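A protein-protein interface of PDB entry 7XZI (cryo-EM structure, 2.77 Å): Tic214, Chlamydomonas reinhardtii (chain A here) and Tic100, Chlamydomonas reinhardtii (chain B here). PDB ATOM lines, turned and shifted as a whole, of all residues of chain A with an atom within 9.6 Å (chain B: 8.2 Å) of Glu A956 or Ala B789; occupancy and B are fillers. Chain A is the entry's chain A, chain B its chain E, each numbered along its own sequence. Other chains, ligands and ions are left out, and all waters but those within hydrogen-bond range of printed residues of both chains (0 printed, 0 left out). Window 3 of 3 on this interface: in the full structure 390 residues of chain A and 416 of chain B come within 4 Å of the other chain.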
ATOM      1  N   PHE A  93      -2.116 -17.534  -6.285  1.00  0.00           N
ATOM      2  CA  PHE A  93      -0.783 -17.662  -5.718  1.00  0.00           C
ATOM      3  C   PHE A  93       0.270 -17.504  -6.808  1.00  0.00           C
ATOM      4  O   PHE A  93       0.051 -17.838  -7.974  1.00  0.00           O
ATOM      5  CB  PHE A  93      -0.612 -19.002  -4.995  1.00  0.00           C
ATOM      6  CG  PHE A  93      -1.096 -20.185  -5.780  1.00  0.00           C
ATOM      7  CD1 PHE A  93      -2.413 -20.602  -5.682  1.00  0.00           C
ATOM      8  CD2 PHE A  93      -0.234 -20.888  -6.603  1.00  0.00           C
ATOM      9  CE1 PHE A  93      -2.863 -21.692  -6.397  1.00  0.00           C
ATOM     10  CE2 PHE A  93      -0.679 -21.980  -7.321  1.00  0.00           C
ATOM     11  CZ  PHE A  93      -1.995 -22.382  -7.217  1.00  0.00           C
ATOM     12  N   GLU A  95       2.472 -18.503  -8.693  1.00  0.00           N
ATOM     13  CA  GLU A  95       3.017 -19.648  -9.441  1.00  0.00           C
ATOM     14  C   GLU A  95       3.842 -20.494  -8.470  1.00  0.00           C
ATOM     15  O   GLU A  95       3.314 -20.915  -7.431  1.00  0.00           O
ATOM     16  CB  GLU A  95       3.762 -19.136 -10.668  1.00  0.00           C
ATOM     17  CG  GLU A  95       4.089 -20.210 -11.700  1.00  0.00           C
ATOM     18  CD  GLU A  95       5.037 -19.715 -12.774  1.00  0.00           C
ATOM     19  OE1 GLU A  95       5.428 -18.531 -12.721  1.00  0.00           O
ATOM     20  OE2 GLU A  95       5.394 -20.511 -13.669  1.00  0.00           O
ATOM     21  N   THR A  96       5.114 -20.761  -8.754  1.00  0.00           N
ATOM     22  CA  THR A  96       5.971 -21.562  -7.894  1.00  0.00           C
ATOM     23  C   THR A  96       7.027 -20.669  -7.261  1.00  0.00           C
ATOM     24  O   THR A  96       7.771 -19.981  -7.968  1.00  0.00           O
ATOM     25  CB  THR A  96       6.642 -22.685  -8.689  1.00  0.00           C
ATOM     26  OG1 THR A  96       5.654 -23.379  -9.461  1.00  0.00           O
ATOM     27  CG2 THR A  96       7.327 -23.669  -7.751  1.00  0.00           C
ATOM     28  N   SER A  97       7.085 -20.676  -5.932  1.00  0.00           N
ATOM     29  CA  SER A  97       8.117 -19.974  -5.177  1.00  0.00           C
ATOM     30  C   SER A  97       8.778 -20.971  -4.238  1.00  0.00           C
ATOM     31  O   SER A  97       8.104 -21.574  -3.396  1.00  0.00           O
ATOM     32  CB  SER A  97       7.530 -18.795  -4.397  1.00  0.00           C
ATOM     33  OG  SER A  97       6.955 -17.840  -5.271  1.00  0.00           O
ATOM     34  N   VAL A  98      10.088 -21.142  -4.382  1.00  0.00           N
ATOM     35  CA  VAL A  98      10.845 -22.108  -3.597  1.00  0.00           C
ATOM     36  C   VAL A  98      12.137 -21.453  -3.130  1.00  0.00           C
ATOM     37  O   VAL A  98      12.766 -20.694  -3.874  1.00  0.00           O
ATOM     38  CB  VAL A  98      11.145 -23.389  -4.404  1.00  0.00           C
ATOM     39  N   ASN A  99      12.526 -21.744  -1.891  1.00  0.00           N
ATOM     40  CA  ASN A  99      13.777 -21.223  -1.359  1.00  0.00           C
ATOM     41  C   ASN A  99      14.952 -21.867  -2.084  1.00  0.00           C
ATOM     42  O   ASN A  99      14.997 -23.090  -2.254  1.00  0.00           O
ATOM     43  N   PRO A 238      10.426 -36.863  -8.454  1.00  0.00           N
ATOM     44  CA  PRO A 238       9.011 -36.632  -8.102  1.00  0.00           C
ATOM     45  C   PRO A 238       8.194 -36.110  -9.279  1.00  0.00           C
ATOM     46  O   PRO A 238       7.564 -35.051  -9.217  1.00  0.00           O
ATOM     47  CB  PRO A 238       9.119 -35.608  -6.961  1.00  0.00           C
ATOM     48  CG  PRO A 238      10.574 -35.564  -6.567  1.00  0.00           C
ATOM     49  CD  PRO A 238      11.319 -35.893  -7.808  1.00  0.00           C
ATOM     50  N   ASN A 950      -6.115 -38.043  10.265  1.00  0.00           N
ATOM     51  CA  ASN A 950      -5.857 -37.144   9.141  1.00  0.00           C
ATOM     52  C   ASN A 950      -5.428 -37.939   7.906  1.00  0.00           C
ATOM     53  O   ASN A 950      -4.314 -37.814   7.398  1.00  0.00           O
ATOM     54  CB  ASN A 950      -4.808 -36.108   9.529  1.00  0.00           C
ATOM     55  N   TYR A 952      -6.902 -37.919   4.756  1.00  0.00           N
ATOM     56  CA  TYR A 952      -6.922 -37.096   3.556  1.00  0.00           C
ATOM     57  C   TYR A 952      -6.234 -35.750   3.743  1.00  0.00           C
ATOM     58  O   TYR A 952      -6.148 -34.977   2.785  1.00  0.00           O
ATOM     59  CB  TYR A 952      -8.367 -36.871   3.096  1.00  0.00           C
ATOM     60  CG  TYR A 952      -9.038 -38.099   2.523  1.00  0.00           C
ATOM     61  CD1 TYR A 952      -9.735 -38.979   3.339  1.00  0.00           C
ATOM     62  CD2 TYR A 952      -8.980 -38.374   1.165  1.00  0.00           C
ATOM     63  CE1 TYR A 952     -10.351 -40.100   2.817  1.00  0.00           C
ATOM     64  CE2 TYR A 952      -9.593 -39.492   0.636  1.00  0.00           C
ATOM     65  CZ  TYR A 952     -10.276 -40.351   1.466  1.00  0.00           C
ATOM     66  OH  TYR A 952     -10.886 -41.465   0.940  1.00  0.00           O
ATOM     67  N   PHE A 953      -5.741 -35.454   4.942  1.00  0.00           N
ATOM     68  CA  PHE A 953      -5.119 -34.169   5.227  1.00  0.00           C
ATOM     69  C   PHE A 953      -3.653 -34.185   4.814  1.00  0.00           C
ATOM     70  O   PHE A 953      -2.928 -35.139   5.112  1.00  0.00           O
ATOM     71  CB  PHE A 953      -5.237 -33.828   6.712  1.00  0.00           C
ATOM     72  CG  PHE A 953      -6.608 -33.375   7.124  1.00  0.00           C
ATOM     73  CD1 PHE A 953      -7.608 -34.297   7.381  1.00  0.00           C
ATOM     74  CD2 PHE A 953      -6.892 -32.028   7.262  1.00  0.00           C
ATOM     75  CE1 PHE A 953      -8.867 -33.883   7.761  1.00  0.00           C
ATOM     76  CE2 PHE A 953      -8.150 -31.608   7.643  1.00  0.00           C
ATOM     77  CZ  PHE A 953      -9.139 -32.537   7.893  1.00  0.00           C
ATOM     78  N   HIS A 954      -3.226 -33.132   4.121  1.00  0.00           N
ATOM     79  CA  HIS A 954      -1.812 -32.957   3.829  1.00  0.00           C
ATOM     80  C   HIS A 954      -1.049 -32.701   5.123  1.00  0.00           C
ATOM     81  O   HIS A 954      -1.517 -31.973   6.003  1.00  0.00           O
ATOM     82  CB  HIS A 954      -1.611 -31.797   2.852  1.00  0.00           C
ATOM     83  CG  HIS A 954      -0.319 -31.855   2.097  1.00  0.00           C
ATOM     84  ND1 HIS A 954       0.884 -31.467   2.647  1.00  0.00           N
ATOM     85  CD2 HIS A 954      -0.044 -32.248   0.831  1.00  0.00           C
ATOM     86  CE1 HIS A 954       1.845 -31.622   1.753  1.00  0.00           C
ATOM     87  NE2 HIS A 954       1.308 -32.095   0.644  1.00  0.00           N
ATOM     88  N   GLU A 955       0.134 -33.308   5.238  1.00  0.00           N
ATOM     89  CA  GLU A 955       0.903 -33.202   6.474  1.00  0.00           C
ATOM     90  C   GLU A 955       1.335 -31.766   6.743  1.00  0.00           C
ATOM     91  O   GLU A 955       1.588 -31.392   7.895  1.00  0.00           O
ATOM     92  CB  GLU A 955       2.118 -34.129   6.422  1.00  0.00           C
ATOM     93  CG  GLU A 955       3.107 -33.811   5.312  1.00  0.00           C
ATOM     94  CD  GLU A 955       4.313 -34.732   5.330  1.00  0.00           C
ATOM     95  OE1 GLU A 955       4.373 -35.620   6.206  1.00  0.00           O
ATOM     96  OE2 GLU A 955       5.201 -34.565   4.467  1.00  0.00           O
ATOM     97  N   GLU A 956       1.431 -30.947   5.696  1.00  0.00           N
ATOM     98  CA  GLU A 956       1.819 -29.554   5.885  1.00  0.00           C
ATOM     99  C   GLU A 956       0.699 -28.753   6.539  1.00  0.00           C
ATOM    100  O   GLU A 956       0.958 -27.780   7.258  1.00  0.00           O
ATOM    101  CB  GLU A 956       2.221 -28.940   4.543  1.00  0.00           C
ATOM    102  CG  GLU A 956       3.054 -27.676   4.659  1.00  0.00           C
ATOM    103  CD  GLU A 956       4.060 -27.538   3.533  1.00  0.00           C
ATOM    104  OE1 GLU A 956       4.410 -28.567   2.918  1.00  0.00           O
ATOM    105  OE2 GLU A 956       4.499 -26.401   3.260  1.00  0.00           O
ATOM    106  N   LEU A 957      -0.555 -29.146   6.299  1.00  0.00           N
ATOM    107  CA  LEU A 957      -1.686 -28.433   6.884  1.00  0.00           C
ATOM    108  C   LEU A 957      -1.845 -28.728   8.371  1.00  0.00           C
ATOM    109  O   LEU A 957      -2.391 -27.901   9.109  1.00  0.00           O
ATOM    110  CB  LEU A 957      -2.974 -28.790   6.141  1.00  0.00           C
ATOM    111  CG  LEU A 957      -3.000 -28.540   4.632  1.00  0.00           C
ATOM    112  CD1 LEU A 957      -4.320 -28.999   4.034  1.00  0.00           C
ATOM    113  CD2 LEU A 957      -2.755 -27.072   4.334  1.00  0.00           C
ATOM    114  N   LEU A 958      -1.389 -29.900   8.825  1.00  0.00           N
ATOM    115  CA  LEU A 958      -1.629 -30.319  10.203  1.00  0.00           C
ATOM    116  C   LEU A 958      -0.948 -29.417  11.225  1.00  0.00           C
ATOM    117  O   LEU A 958      -1.384 -29.372  12.381  1.00  0.00           O
ATOM    118  CB  LEU A 958      -1.161 -31.763  10.396  1.00  0.00           C
ATOM    119  CG  LEU A 958      -1.878 -32.800   9.529  1.00  0.00           C
ATOM    120  CD1 LEU A 958      -1.359 -34.201   9.813  1.00  0.00           C
ATOM    121  CD2 LEU A 958      -3.379 -32.724   9.750  1.00  0.00           C
ATOM    122  N   THR A 959       0.102 -28.704  10.835  1.00  0.00           N
ATOM    123  CA  THR A 959       0.793 -27.811  11.758  1.00  0.00           C
ATOM    124  C   THR A 959       0.048 -26.488  11.897  1.00  0.00           C
ATOM    125  O   THR A 959      -1.102 -26.455  12.336  1.00  0.00           O
ATOM    126  CB  THR A 959       2.238 -27.537  11.304  1.00  0.00           C
ATOM    127  OG1 THR A 959       2.229 -26.948   9.998  1.00  0.00           O
ATOM    128  CG2 THR A 959       3.037 -28.830  11.266  1.00  0.00           C
ATOM    129  N   GLY B 775       4.119 -25.966 -10.788  1.00  0.00           N
ATOM    130  CA  GLY B 775       4.275 -26.213  -9.362  1.00  0.00           C
ATOM    131  C   GLY B 775       2.973 -26.418  -8.620  1.00  0.00           C
ATOM    132  O   GLY B 775       2.808 -25.903  -7.507  1.00  0.00           O
ATOM    133  N   THR B 776       2.040 -27.161  -9.211  1.00  0.00           N
ATOM    134  CA  THR B 776       0.775 -27.493  -8.570  1.00  0.00           C
ATOM    135  C   THR B 776       0.676 -28.984  -8.268  1.00  0.00           C
ATOM    136  O   THR B 776      -0.424 -29.531  -8.163  1.00  0.00           O
ATOM    137  CB  THR B 776      -0.406 -27.050  -9.433  1.00  0.00           C
ATOM    138  OG1 THR B 776      -0.353 -27.724 -10.696  1.00  0.00           O
ATOM    139  CG2 THR B 776      -0.373 -25.548  -9.662  1.00  0.00           C
ATOM    140  N   LYS B 777       1.821 -29.654  -8.128  1.00  0.00           N
ATOM    141  CA  LYS B 777       1.827 -31.088  -7.871  1.00  0.00           C
ATOM    142  C   LYS B 777       1.331 -31.438  -6.476  1.00  0.00           C
ATOM    143  O   LYS B 777       1.089 -32.619  -6.205  1.00  0.00           O
ATOM    144  CB  LYS B 777       3.232 -31.656  -8.076  1.00  0.00           C
ATOM    145  CG  LYS B 777       3.846 -31.306  -9.420  1.00  0.00           C
ATOM    146  CD  LYS B 777       5.147 -32.056  -9.652  1.00  0.00           C
ATOM    147  CE  LYS B 777       5.836 -31.570 -10.917  1.00  0.00           C
ATOM    148  NZ  LYS B 777       4.937 -31.649 -12.101  1.00  0.00           N
ATOM    149  N   PHE B 778       1.178 -30.453  -5.589  1.00  0.00           N
ATOM    150  CA  PHE B 778       0.597 -30.708  -4.278  1.00  0.00           C
ATOM    151  C   PHE B 778      -0.883 -31.053  -4.355  1.00  0.00           C
ATOM    152  O   PHE B 778      -1.441 -31.535  -3.365  1.00  0.00           O
ATOM    153  CB  PHE B 778       0.802 -29.498  -3.364  1.00  0.00           C
ATOM    154  CG  PHE B 778       0.011 -28.285  -3.771  1.00  0.00           C
ATOM    155  CD1 PHE B 778       0.489 -27.423  -4.742  1.00  0.00           C
ATOM    156  CD2 PHE B 778      -1.207 -28.003  -3.173  1.00  0.00           C
ATOM    157  CE1 PHE B 778      -0.236 -26.306  -5.115  1.00  0.00           C
ATOM    158  CE2 PHE B 778      -1.934 -26.891  -3.542  1.00  0.00           C
ATOM    159  CZ  PHE B 778      -1.449 -26.041  -4.514  1.00  0.00           C
ATOM    160  N   MET B 779      -1.526 -30.818  -5.500  1.00  0.00           N
ATOM    161  CA  MET B 779      -2.931 -31.157  -5.676  1.00  0.00           C
ATOM    162  C   MET B 779      -3.148 -32.625  -6.013  1.00  0.00           C
ATOM    163  O   MET B 779      -4.302 -33.059  -6.085  1.00  0.00           O
ATOM    164  CB  MET B 779      -3.549 -30.292  -6.777  1.00  0.00           C
ATOM    165  CG  MET B 779      -3.450 -28.799  -6.529  1.00  0.00           C
ATOM    166  SD  MET B 779      -4.195 -27.836  -7.858  1.00  0.00           S
ATOM    167  CE  MET B 779      -3.949 -26.172  -7.242  1.00  0.00           C
ATOM    168  N   LEU B 784       2.370 -38.682  -4.337  1.00  0.00           N
ATOM    169  CA  LEU B 784       3.142 -37.657  -5.033  1.00  0.00           C
ATOM    170  C   LEU B 784       2.865 -36.274  -4.460  1.00  0.00           C
ATOM    171  O   LEU B 784       3.749 -35.410  -4.451  1.00  0.00           O
ATOM    172  CB  LEU B 784       2.828 -37.690  -6.529  1.00  0.00           C
ATOM    173  CG  LEU B 784       3.663 -36.780  -7.433  1.00  0.00           C
ATOM    174  CD1 LEU B 784       5.072 -37.332  -7.596  1.00  0.00           C
ATOM    175  CD2 LEU B 784       2.993 -36.581  -8.786  1.00  0.00           C
ATOM    176  N   GLY B 785       1.641 -36.043  -3.985  1.00  0.00           N
ATOM    177  CA  GLY B 785       1.303 -34.739  -3.438  1.00  0.00           C
ATOM    178  C   GLY B 785       2.065 -34.414  -2.167  1.00  0.00           C
ATOM    179  O   GLY B 785       2.441 -33.262  -1.935  1.00  0.00           O
ATOM    180  N   LEU B 786       2.300 -35.422  -1.324  1.00  0.00           N
ATOM    181  CA  LEU B 786       2.993 -35.187  -0.061  1.00  0.00           C
ATOM    182  C   LEU B 786       4.445 -34.783  -0.285  1.00  0.00           C
ATOM    183  O   LEU B 786       5.049 -34.118   0.564  1.00  0.00           O
ATOM    184  CB  LEU B 786       2.915 -36.432   0.820  1.00  0.00           C
ATOM    185  CG  LEU B 786       1.518 -36.883   1.242  1.00  0.00           C
ATOM    186  CD1 LEU B 786       1.606 -37.996   2.271  1.00  0.00           C
ATOM    187  CD2 LEU B 786       0.724 -35.708   1.787  1.00  0.00           C
ATOM    188  N   CYS B 787       5.026 -35.180  -1.420  1.00  0.00           N
ATOM    189  CA  CYS B 787       6.419 -34.843  -1.696  1.00  0.00           C
ATOM    190  C   CYS B 787       6.621 -33.344  -1.868  1.00  0.00           C
ATOM    191  O   CYS B 787       7.686 -32.817  -1.529  1.00  0.00           O
ATOM    192  CB  CYS B 787       6.899 -35.590  -2.940  1.00  0.00           C
ATOM    193  SG  CYS B 787       6.813 -37.388  -2.793  1.00  0.00           S
ATOM    194  N   HIS B 788       5.619 -32.642  -2.388  1.00  0.00           N
ATOM    195  CA  HIS B 788       5.709 -31.213  -2.646  1.00  0.00           C
ATOM    196  C   HIS B 788       4.984 -30.426  -1.558  1.00  0.00           C
ATOM    197  O   HIS B 788       4.236 -30.976  -0.748  1.00  0.00           O
ATOM    198  CB  HIS B 788       5.138 -30.887  -4.028  1.00  0.00           C
ATOM    199  CG  HIS B 788       5.807 -31.633  -5.140  1.00  0.00           C
ATOM    200  ND1 HIS B 788       6.827 -31.092  -5.891  1.00  0.00           N
ATOM    201  CD2 HIS B 788       5.613 -32.885  -5.617  1.00  0.00           C
ATOM    202  CE1 HIS B 788       7.226 -31.975  -6.789  1.00  0.00           C
ATOM    203  NE2 HIS B 788       6.506 -33.071  -6.642  1.00  0.00           N
ATOM    204  N   ALA B 789       5.217 -29.118  -1.553  1.00  0.00           N
ATOM    205  CA  ALA B 789       4.727 -28.231  -0.510  1.00  0.00           C
ATOM    206  C   ALA B 789       3.617 -27.332  -1.037  1.00  0.00           C
ATOM    207  O   ALA B 789       3.518 -27.058  -2.235  1.00  0.00           O
ATOM    208  CB  ALA B 789       5.864 -27.375   0.057  1.00  0.00           C
ATOM    209  N   VAL B 790       2.780 -26.871  -0.113  1.00  0.00           N
ATOM    210  CA  VAL B 790       1.656 -25.992  -0.428  1.00  0.00           C
ATOM    211  C   VAL B 790       2.165 -24.561  -0.580  1.00  0.00           C
ATOM    212  O   VAL B 790       3.205 -24.210  -0.004  1.00  0.00           O
ATOM    213  CB  VAL B 790       0.565 -26.094   0.648  1.00  0.00           C
ATOM    214  CG1 VAL B 790      -0.071 -27.475   0.616  1.00  0.00           C
ATOM    215  CG2 VAL B 790       1.153 -25.813   2.019  1.00  0.00           C
ATOM    216  N   PRO B 791       1.477 -23.704  -1.337  1.00  0.00           N
ATOM    217  CA  PRO B 791       1.989 -22.355  -1.609  1.00  0.00           C
ATOM    218  C   PRO B 791       1.888 -21.378  -0.446  1.00  0.00           C
ATOM    219  O   PRO B 791       2.127 -20.185  -0.653  1.00  0.00           O
ATOM    220  CB  PRO B 791       1.107 -21.884  -2.781  1.00  0.00           C
ATOM    221  CG  PRO B 791       0.479 -23.125  -3.336  1.00  0.00           C
ATOM    222  CD  PRO B 791       0.296 -24.014  -2.157  1.00  0.00           C
ATOM    223  N   ASP B 792       1.540 -21.839   0.759  1.00  0.00           N
ATOM    224  CA  ASP B 792       1.508 -20.995   1.959  1.00  0.00           C
ATOM    225  C   ASP B 792       0.506 -19.850   1.819  1.00  0.00           C
ATOM    226  O   ASP B 792       0.870 -18.672   1.863  1.00  0.00           O
ATOM    227  CB  ASP B 792       2.904 -20.460   2.300  1.00  0.00           C
ATOM    228  CG  ASP B 792       2.971 -19.828   3.683  1.00  0.00           C
ATOM    229  OD1 ASP B 792       1.992 -19.950   4.449  1.00  0.00           O
ATOM    230  OD2 ASP B 792       4.006 -19.207   4.004  1.00  0.00           O
ATOM    231  N   LEU B 796      -6.250 -20.791   0.952  1.00  0.00           N
ATOM    232  CA  LEU B 796      -6.059 -22.060   0.261  1.00  0.00           C
ATOM    233  C   LEU B 796      -5.971 -23.212   1.254  1.00  0.00           C
ATOM    234  O   LEU B 796      -6.516 -24.296   1.013  1.00  0.00           O
ATOM    235  CB  LEU B 796      -4.803 -21.996  -0.609  1.00  0.00           C
ATOM    236  CG  LEU B 796      -4.618 -23.086  -1.665  1.00  0.00           C
ATOM    237  CD1 LEU B 796      -5.722 -23.012  -2.706  1.00  0.00           C
ATOM    238  CD2 LEU B 796      -3.252 -22.975  -2.323  1.00  0.00           C
ATOM    239  N   ARG B 797      -5.285 -22.995   2.380  1.00  0.00           N
ATOM    240  CA  ARG B 797      -5.187 -24.030   3.405  1.00  0.00           C
ATOM    241  C   ARG B 797      -6.551 -24.351   4.001  1.00  0.00           C
ATOM    242  O   ARG B 797      -6.868 -25.522   4.238  1.00  0.00           O
ATOM    243  CB  ARG B 797      -4.213 -23.594   4.498  1.00  0.00           C
ATOM    244  CG  ARG B 797      -2.782 -23.418   4.022  1.00  0.00           C
ATOM    245  CD  ARG B 797      -1.873 -22.974   5.155  1.00  0.00           C
ATOM    246  NE  ARG B 797      -0.499 -22.788   4.711  1.00  0.00           N
ATOM    247  CZ  ARG B 797       0.437 -23.729   4.756  1.00  0.00           C
ATOM    248  NH1 ARG B 797       0.177 -24.941   5.218  1.00  0.00           N
ATOM    249  NH2 ARG B 797       1.663 -23.444   4.330  1.00  0.00           N
ATOM    250  N   MET B 800      -8.474 -26.400   1.438  1.00  0.00           N
ATOM    251  CA  MET B 800      -7.990 -27.777   1.424  1.00  0.00           C
ATOM    252  C   MET B 800      -8.458 -28.537   2.656  1.00  0.00           C
ATOM    253  O   MET B 800      -8.800 -29.722   2.569  1.00  0.00           O
ATOM    254  CB  MET B 800      -6.465 -27.802   1.325  1.00  0.00           C
ATOM    255  CG  MET B 800      -5.913 -27.271   0.015  1.00  0.00           C
ATOM    256  SD  MET B 800      -4.120 -27.415  -0.092  1.00  0.00           S
ATOM    257  CE  MET B 800      -3.919 -29.193  -0.041  1.00  0.00           C
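OG1 of Thr A96 sits close to N of Gly B775, 3.3 Å away. A ring nitrogen (NE2) of His A954 sits at hydrogen-bond distance from the backbone carbonyl oxygen (O) of Gly B785 (3.0 Å). The backbone carbonyl oxygen (O) of Pro A238 sits at hydrogen-bond distance from a ring nitrogen (NE2) of His B788 (3.4 Å). The backbone carbonyl oxygen of His B788 sits at hydrogen-bond distance from a ring nitrogen (NE2) of His A954.
Among the printed residues, merely in contact across the chains: Pro A238 with Lys B777 (3.9 Å), Pro A238 with Leu B784 (3.7 Å), His A954 with Leu B786 (3.6 Å), Glu A955 with Leu B786 (3.9 Å), Glu A956 with Ala B789 (3.4 Å), Glu A956 with Val B790 (3.6 Å), Glu A956 with Arg B797 (3.6 Å), Leu A957 with Arg B797 (3.7 Å) and Leu A957 with Met B800 (3.7 Å).
Glu A956 touches three residues of chain B. Of the printed residues of chain A, Gly B775 touches Thr A96 (3.2 Å). Printed residues of chain A within 4 Å of Gly B785: His A954. Of the printed residues of chain A, Leu B786 touches His A954 and Glu A955. Ala B789 touches one residue of chain A.
Hydrophobic or aromatic side chains of chain B within 4 Å of the printed part of chain A: Leu B784, Leu B786, His B788, Ala B789, Val B790 and Met B800. Of the 16 printed residues of chain A, 6 touch a printed residue of chain B. Printed residues of chain A that touch a printed residue of chain B: Thr A96, Pro A238, His A954, Glu A955, Glu A956 and Leu A957. Hydrophobic or aromatic side chains of chain A within 4 Å of the printed part of chain B: Pro A238, His A954 and Leu A957. Along chain A the printed residues that touch a printed residue of chain B span positions 96 to 957.
The guanidinium group of Arg B797 is in salt-bridge range of the side-chain carboxylate of Asp B792 (3.5 Å). A ring nitrogen (ND1) of His A954 lies close to the backbone NH (N) of Glu A956. The backbone carbonyl oxygen (O) of Glu A956 lies within hydrogen-bond range of the side-chain hydroxyl (OG1) of Thr A959 (3.1 Å).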
